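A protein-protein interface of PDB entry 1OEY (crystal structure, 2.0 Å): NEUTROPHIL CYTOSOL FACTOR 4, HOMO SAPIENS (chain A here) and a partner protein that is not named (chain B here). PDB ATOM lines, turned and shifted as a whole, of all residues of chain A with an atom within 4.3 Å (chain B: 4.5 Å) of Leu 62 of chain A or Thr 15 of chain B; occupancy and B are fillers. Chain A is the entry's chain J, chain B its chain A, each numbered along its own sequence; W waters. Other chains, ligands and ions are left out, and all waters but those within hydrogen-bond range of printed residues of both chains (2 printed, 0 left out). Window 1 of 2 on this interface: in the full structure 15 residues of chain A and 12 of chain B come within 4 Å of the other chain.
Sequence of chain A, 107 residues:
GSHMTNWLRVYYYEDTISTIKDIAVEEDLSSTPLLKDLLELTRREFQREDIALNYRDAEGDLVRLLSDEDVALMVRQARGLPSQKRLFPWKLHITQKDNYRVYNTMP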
ATOM      1  N   TYR A  13      23.710  16.248   8.679  1.00  0.00           N
ATOM      2  CA  TYR A  13      22.599  16.884   7.983  1.00  0.00           C
ATOM      3  C   TYR A  13      21.247  16.663   8.646  1.00  0.00           C
ATOM      4  O   TYR A  13      20.891  15.545   9.002  1.00  0.00           O
ATOM      5  CB  TYR A  13      22.510  16.419   6.538  1.00  0.00           C
ATOM      6  CG  TYR A  13      23.619  16.901   5.648  1.00  0.00           C
ATOM      7  CD1 TYR A  13      23.401  17.866   4.678  1.00  0.00           C
ATOM      8  CD2 TYR A  13      24.884  16.365   5.741  1.00  0.00           C
ATOM      9  CE1 TYR A  13      24.420  18.278   3.841  1.00  0.00           C
ATOM     10  CE2 TYR A  13      25.904  16.790   4.907  1.00  0.00           C
ATOM     11  CZ  TYR A  13      25.653  17.728   3.968  1.00  0.00           C
ATOM     12  OH  TYR A  13      26.656  18.117   3.143  1.00  0.00           O
ATOM     13  N   ASN A  54      28.706   9.819   3.324  1.00  0.00           N
ATOM     14  CA  ASN A  54      28.903  10.431   2.010  1.00  0.00           C
ATOM     15  C   ASN A  54      30.128  11.325   1.998  1.00  0.00           C
ATOM     16  O   ASN A  54      30.641  11.699   3.027  1.00  0.00           O
ATOM     17  CB  ASN A  54      27.716  11.314   1.581  1.00  0.00           C
ATOM     18  CG  ASN A  54      26.342  10.692   1.821  1.00  0.00           C
ATOM     19  OD1 ASN A  54      25.682  10.164   0.881  1.00  0.00           O
ATOM     20  ND2 ASN A  54      25.859  10.821   3.040  1.00  0.00           N
ATOM     21  N   TYR A  55      30.573  11.695   0.813  1.00  0.00           N
ATOM     22  CA  TYR A  55      31.547  12.758   0.637  1.00  0.00           C
ATOM     23  C   TYR A  55      31.111  13.628  -0.510  1.00  0.00           C
ATOM     24  O   TYR A  55      30.267  13.239  -1.305  1.00  0.00           O
ATOM     25  CB  TYR A  55      32.971  12.193   0.382  1.00  0.00           C
ATOM     26  CG  TYR A  55      33.116  11.430  -0.911  1.00  0.00           C
ATOM     27  CD1 TYR A  55      33.706  12.016  -2.039  1.00  0.00           C
ATOM     28  CD2 TYR A  55      32.667  10.117  -1.010  1.00  0.00           C
ATOM     29  CE1 TYR A  55      33.815  11.306  -3.244  1.00  0.00           C
ATOM     30  CE2 TYR A  55      32.774   9.403  -2.196  1.00  0.00           C
ATOM     31  CZ  TYR A  55      33.328  10.000  -3.309  1.00  0.00           C
ATOM     32  OH  TYR A  55      33.440   9.262  -4.469  1.00  0.00           O
ATOM     33  N   ARG A  56      31.656  14.834  -0.586  1.00  0.00           N
ATOM     34  CA  ARG A  56      31.354  15.717  -1.708  1.00  0.00           C
ATOM     35  C   ARG A  56      32.490  15.643  -2.709  1.00  0.00           C
ATOM     36  O   ARG A  56      33.630  15.885  -2.351  1.00  0.00           O
ATOM     37  CB  ARG A  56      31.140  17.187  -1.244  1.00  0.00           C
ATOM     38  CG  ARG A  56      30.317  18.010  -2.249  1.00  0.00           C
ATOM     39  CD  ARG A  56      29.775  19.359  -1.724  1.00  0.00           C
ATOM     40  NE  ARG A  56      28.757  19.229  -0.680  1.00  0.00           N
ATOM     41  CZ  ARG A  56      27.475  18.892  -0.874  1.00  0.00           C
ATOM     42  NH1 ARG A  56      26.996  18.623  -2.086  1.00  0.00           N
ATOM     43  NH2 ARG A  56      26.664  18.835   0.163  1.00  0.00           N
ATOM     44  N   GLY A  60      31.201  19.074  -6.855  1.00  0.00           N
ATOM     45  CA  GLY A  60      30.206  19.530  -5.901  1.00  0.00           C
ATOM     46  C   GLY A  60      29.043  18.573  -5.617  1.00  0.00           C
ATOM     47  O   GLY A  60      28.124  18.956  -4.909  1.00  0.00           O
ATOM     48  N   ASP A  61      29.051  17.353  -6.156  1.00  0.00           N
ATOM     49  CA  ASP A  61      27.948  16.413  -5.903  1.00  0.00           C
ATOM     50  C   ASP A  61      28.240  15.559  -4.693  1.00  0.00           C
ATOM     51  O   ASP A  61      29.362  15.083  -4.510  1.00  0.00           O
ATOM     52  CB  ASP A  61      27.710  15.465  -7.084  1.00  0.00           C
ATOM     53  CG  ASP A  61      27.200  16.146  -8.304  1.00  0.00           C
ATOM     54  OD1 ASP A  61      26.638  17.279  -8.214  1.00  0.00           O
ATOM     55  OD2 ASP A  61      27.326  15.591  -9.428  1.00  0.00           O
ATOM     56  N   LEU A  62      27.231  15.335  -3.873  1.00  0.00           N
ATOM     57  CA  LEU A  62      27.361  14.451  -2.729  1.00  0.00           C
ATOM     58  C   LEU A  62      27.249  13.033  -3.240  1.00  0.00           C
ATOM     59  O   LEU A  62      26.386  12.733  -4.074  1.00  0.00           O
ATOM     60  CB  LEU A  62      26.279  14.731  -1.700  1.00  0.00           C
ATOM     61  CG  LEU A  62      26.507  14.176  -0.310  1.00  0.00           C
ATOM     62  CD1 LEU A  62      27.593  14.998   0.388  1.00  0.00           C
ATOM     63  CD2 LEU A  62      25.223  14.218   0.520  1.00  0.00           C
ATOM     64  N   VAL A  63      28.128  12.175  -2.748  1.00  0.00           N
ATOM     65  CA  VAL A  63      28.239  10.794  -3.197  1.00  0.00           C
ATOM     66  C   VAL A  63      28.117   9.899  -1.991  1.00  0.00           C
ATOM     67  O   VAL A  63      28.821  10.073  -1.013  1.00  0.00           O
ATOM     68  CB  VAL A  63      29.595  10.561  -3.898  1.00  0.00           C
ATOM     69  CG1 VAL A  63      29.793   9.108  -4.308  1.00  0.00           C
ATOM     70  CG2 VAL A  63      29.714  11.449  -5.123  1.00  0.00           C
ATOM     71  N   ARG A  64      27.207   8.934  -2.053  1.00  0.00           N
ATOM     72  CA  ARG A  64      27.027   7.982  -0.974  1.00  0.00           C
ATOM     73  C   ARG A  64      28.114   6.900  -1.027  1.00  0.00           C
ATOM     74  O   ARG A  64      28.447   6.364  -2.086  1.00  0.00           O
ATOM     75  CB  ARG A  64      25.612   7.372  -1.036  1.00  0.00           C
ATOM     76  CG  ARG A  64      25.301   6.334   0.056  1.00  0.00           C
ATOM     77  CD  ARG A  64      23.889   5.816   0.052  1.00  0.00           C
ATOM     78  NE  ARG A  64      22.915   6.850   0.395  1.00  0.00           N
ATOM     79  CZ  ARG A  64      21.691   6.612   0.830  1.00  0.00           C
ATOM     80  NH1 ARG A  64      21.246   5.373   0.909  1.00  0.00           N
ATOM     81  NH2 ARG A  64      20.906   7.613   1.156  1.00  0.00           N
ATOM     82  N   HIS A  93      30.298  13.319   5.420  1.00  0.00           N
ATOM     83  CA  HIS A  93      28.954  13.842   5.369  1.00  0.00           C
ATOM     84  C   HIS A  93      27.964  12.742   5.785  1.00  0.00           C
ATOM     85  O   HIS A  93      27.888  11.686   5.126  1.00  0.00           O
ATOM     86  CB  HIS A  93      28.623  14.334   3.950  1.00  0.00           C
ATOM     87  CG  HIS A  93      29.473  15.473   3.485  1.00  0.00           C
ATOM     88  ND1 HIS A  93      28.978  16.748   3.295  1.00  0.00           N
ATOM     89  CD2 HIS A  93      30.789  15.531   3.178  1.00  0.00           C
ATOM     90  CE1 HIS A  93      29.950  17.531   2.866  1.00  0.00           C
ATOM     91  NE2 HIS A  93      31.066  16.828   2.824  1.00  0.00           N
ATOM     92  N   VAL A 102      19.484  15.799  -0.523  1.00  0.00           N
ATOM     93  CA  VAL A 102      20.866  16.274  -0.519  1.00  0.00           C
ATOM     94  C   VAL A 102      21.684  15.881  -1.758  1.00  0.00           C
ATOM     95  O   VAL A 102      22.758  16.412  -1.967  1.00  0.00           O
ATOM     96  CB  VAL A 102      21.626  15.747   0.722  1.00  0.00           C
ATOM     97  CG1 VAL A 102      21.106  16.371   1.968  1.00  0.00           C
ATOM     98  CG2 VAL A 102      21.539  14.230   0.801  1.00  0.00           C
ATOM     99  N   TYR A 103      21.153  14.991  -2.586  1.00  0.00           N
ATOM    100  CA  TYR A 103      21.858  14.478  -3.745  1.00  0.00           C
ATOM    101  C   TYR A 103      21.468  15.278  -4.979  1.00  0.00           C
ATOM    102  O   TYR A 103      20.303  15.602  -5.131  1.00  0.00           O
ATOM    103  CB  TYR A 103      21.526  12.985  -3.920  1.00  0.00           C
ATOM    104  CG  TYR A 103      21.994  12.121  -2.740  1.00  0.00           C
ATOM    105  CD1 TYR A 103      23.350  11.878  -2.527  1.00  0.00           C
ATOM    106  CD2 TYR A 103      21.084  11.545  -1.859  1.00  0.00           C
ATOM    107  CE1 TYR A 103      23.790  11.108  -1.480  1.00  0.00           C
ATOM    108  CE2 TYR A 103      21.508  10.781  -0.783  1.00  0.00           C
ATOM    109  CZ  TYR A 103      22.870  10.559  -0.603  1.00  0.00           C
ATOM    110  OH  TYR A 103      23.314   9.803   0.452  1.00  0.00           O
ATOM    111  N   THR A 105      20.723  14.817  -8.122  1.00  0.00           N
ATOM    112  CA  THR A 105      20.239  13.822  -9.066  1.00  0.00           C
ATOM    113  C   THR A 105      19.357  14.382 -10.182  1.00  0.00           C
ATOM    114  O   THR A 105      18.960  13.648 -11.070  1.00  0.00           O
ATOM    115  CB  THR A 105      19.434  12.715  -8.345  1.00  0.00           C
ATOM    116  OG1 THR A 105      18.357  13.307  -7.625  1.00  0.00           O
ATOM    117  CG2 THR A 105      20.286  11.966  -7.290  1.00  0.00           C
ATOM    118  N   LYS B   9      29.480   7.959 -12.846  1.00  0.00           N
ATOM    119  CA  LYS B   9      28.676   8.540 -11.777  1.00  0.00           C
ATOM    120  C   LYS B   9      27.217   8.266 -12.108  1.00  0.00           C
ATOM    121  O   LYS B   9      26.772   8.553 -13.226  1.00  0.00           O
ATOM    122  CB  LYS B   9      28.963  10.029 -11.632  1.00  0.00           C
ATOM    123  CG  LYS B   9      27.896  10.798 -10.885  1.00  0.00           C
ATOM    124  CD  LYS B   9      28.428  11.861  -9.976  1.00  0.00           C
ATOM    125  CE  LYS B   9      28.918  13.038 -10.705  1.00  0.00           C
ATOM    126  NZ  LYS B   9      29.727  13.983  -9.852  1.00  0.00           N
ATOM    127  N   VAL B  10      26.477   7.701 -11.147  1.00  0.00           N
ATOM    128  CA  VAL B  10      25.088   7.324 -11.372  1.00  0.00           C
ATOM    129  C   VAL B  10      24.180   8.013 -10.396  1.00  0.00           C
ATOM    130  O   VAL B  10      24.343   7.872  -9.208  1.00  0.00           O
ATOM    131  CB  VAL B  10      24.845   5.800 -11.247  1.00  0.00           C
ATOM    132  CG1 VAL B  10      23.407   5.495 -11.569  1.00  0.00           C
ATOM    133  CG2 VAL B  10      25.780   5.017 -12.179  1.00  0.00           C
ATOM    134  N   HIS B  11      23.192   8.723 -10.913  1.00  0.00           N
ATOM    135  CA  HIS B  11      22.201   9.370 -10.075  1.00  0.00           C
ATOM    136  C   HIS B  11      20.934   8.544 -10.022  1.00  0.00           C
ATOM    137  O   HIS B  11      20.149   8.497 -10.973  1.00  0.00           O
ATOM    138  CB  HIS B  11      21.881  10.746 -10.627  1.00  0.00           C
ATOM    139  CG  HIS B  11      23.028  11.711 -10.564  1.00  0.00           C
ATOM    140  ND1 HIS B  11      23.612  12.090  -9.377  1.00  0.00           N
ATOM    141  CD2 HIS B  11      23.621  12.445 -11.532  1.00  0.00           C
ATOM    142  CE1 HIS B  11      24.542  12.999  -9.625  1.00  0.00           C
ATOM    143  NE2 HIS B  11      24.551  13.244 -10.924  1.00  0.00           N
ATOM    144  N   TYR B  14      19.835   8.244  -4.629  1.00  0.00           N
ATOM    145  CA  TYR B  14      21.139   8.763  -4.184  1.00  0.00           C
ATOM    146  C   TYR B  14      22.139   8.618  -5.324  1.00  0.00           C
ATOM    147  O   TYR B  14      21.859   7.965  -6.333  1.00  0.00           O
ATOM    148  CB  TYR B  14      21.646   8.004  -2.929  1.00  0.00           C
ATOM    149  CG  TYR B  14      21.643   6.488  -3.044  1.00  0.00           C
ATOM    150  CD1 TYR B  14      22.735   5.816  -3.532  1.00  0.00           C
ATOM    151  CD2 TYR B  14      20.519   5.735  -2.689  1.00  0.00           C
ATOM    152  CE1 TYR B  14      22.741   4.415  -3.644  1.00  0.00           C
ATOM    153  CE2 TYR B  14      20.504   4.316  -2.809  1.00  0.00           C
ATOM    154  CZ  TYR B  14      21.636   3.681  -3.285  1.00  0.00           C
ATOM    155  OH  TYR B  14      21.679   2.320  -3.434  1.00  0.00           O
ATOM    156  N   THR B  15      23.308   9.216  -5.157  1.00  0.00           N
ATOM    157  CA  THR B  15      24.341   9.233  -6.168  1.00  0.00           C
ATOM    158  C   THR B  15      25.478   8.312  -5.749  1.00  0.00           C
ATOM    159  O   THR B  15      25.832   8.289  -4.593  1.00  0.00           O
ATOM    160  CB  THR B  15      24.873  10.656  -6.291  1.00  0.00           C
ATOM    161  OG1 THR B  15      23.849  11.531  -6.777  1.00  0.00           O
ATOM    162  CG2 THR B  15      25.980  10.774  -7.316  1.00  0.00           C
ATOM    163  N   VAL B  16      26.031   7.568  -6.700  1.00  0.00           N
ATOM    164  CA  VAL B  16      27.186   6.711  -6.462  1.00  0.00           C
ATOM    165  C   VAL B  16      28.212   6.968  -7.530  1.00  0.00           C
ATOM    166  O   VAL B  16      27.913   7.537  -8.584  1.00  0.00           O
ATOM    167  CB  VAL B  16      26.839   5.182  -6.436  1.00  0.00           C
ATOM    168  CG1 VAL B  16      25.880   4.907  -5.336  1.00  0.00           C
ATOM    169  CG2 VAL B  16      26.250   4.691  -7.756  1.00  0.00           C
HETATM  170  O   HOH W   1      26.259  15.442 -11.917  1.00  0.00           O
HETATM  171  O   HOH W   2      24.707  13.990  -5.801  1.00  0.00           O
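The side-chain amino group of Lys 9 of chain B lies within salt-bridge range of the side-chain carboxylate of Asp 61 of chain A, at 2.9 Å.
O of Thr 15 of chain B sits at hydrogen-bond distance from N of Arg 64 of chain A (3.0 Å).
A ring nitrogen (ND1) of His 11 of chain B is in hydrogen-bond range of the side-chain hydroxyl of Thr 15 of chain B (2.7 Å).
OH of Tyr 103 of chain A lies within hydrogen-bond range of OD1 of Asn 54 of chain A.
The backbone carbonyl oxygen of Tyr 55 of chain A lies within hydrogen-bond range of the backbone NH of Val 63 of chain A, at 2.8 Å.
NE of Arg 64 of chain A sits at hydrogen-bond distance from OH of Tyr 103 of chain A, at 3.0 Å.
Among the printed residues, merely in contact across the chains: Asp 61 of chain A with His 11 of chain B (3.8 Å), Leu 62 of chain A with Thr 15 of chain B (3.4 Å), Val 63 of chain A with Thr 15 of chain B (3.7 Å), Arg 64 of chain A with Tyr 14 of chain B (3.7 Å), Tyr 103 of chain A with Tyr 14 of chain B (3.5 Å), Tyr 103 of chain A with Thr 15 of chain B (3.7 Å), Thr 105 of chain A with His 11 of chain B (3.8 Å) and Thr 105 of chain A with Thr 15 of chain B (3.6 Å).
Of chain B, only Thr 15 comes within 4 Å of Leu 62 of chain A.
Of the printed residues of chain B, Tyr 103 of chain A touches Tyr 14 (3.5 Å) and Thr 15 (3.7 Å).
Of the printed residues of chain A, His 11 of chain B touches Asp 61 (3.8 Å) and Thr 105 (3.8 Å).
Thr 15 of chain B touches five residues of chain A.
The nearest printed residue of chain B that does not touch Leu 62 of chain A is Val 16 of chain B (5.8 Å).
The nearest printed residue of chain A that does not touch Thr 15 of chain B is Asp 61 of chain A (5.0 Å).
Of the 13 printed residues of chain A, 6 touch a printed residue of chain B.
Hydrophobic or aromatic side chains of chain A within 4 Å of the printed part of chain B: Tyr 103.
Printed residues of chain B that touch a printed residue of chain A: Lys 9, His 11, Tyr 14 and Thr 15.
Hydrophobic or aromatic side chains of chain B that line the printed part of chain A: His 11 and Tyr 14.
Along chain B the printed residues that touch a printed residue of chain A span positions 9 to 15.
Among the printed residues, 10 pairs touch across the chains.
Water W1 lies within hydrogen-bond range of the side-chain carboxylate (OD2) of Asp 61 of chain A and a ring nitrogen (NE2) of His 11 of chain B.
Water W2 lies within hydrogen-bond range of O of Leu 62 of chain A and OG1 of Thr 15 of chain B.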
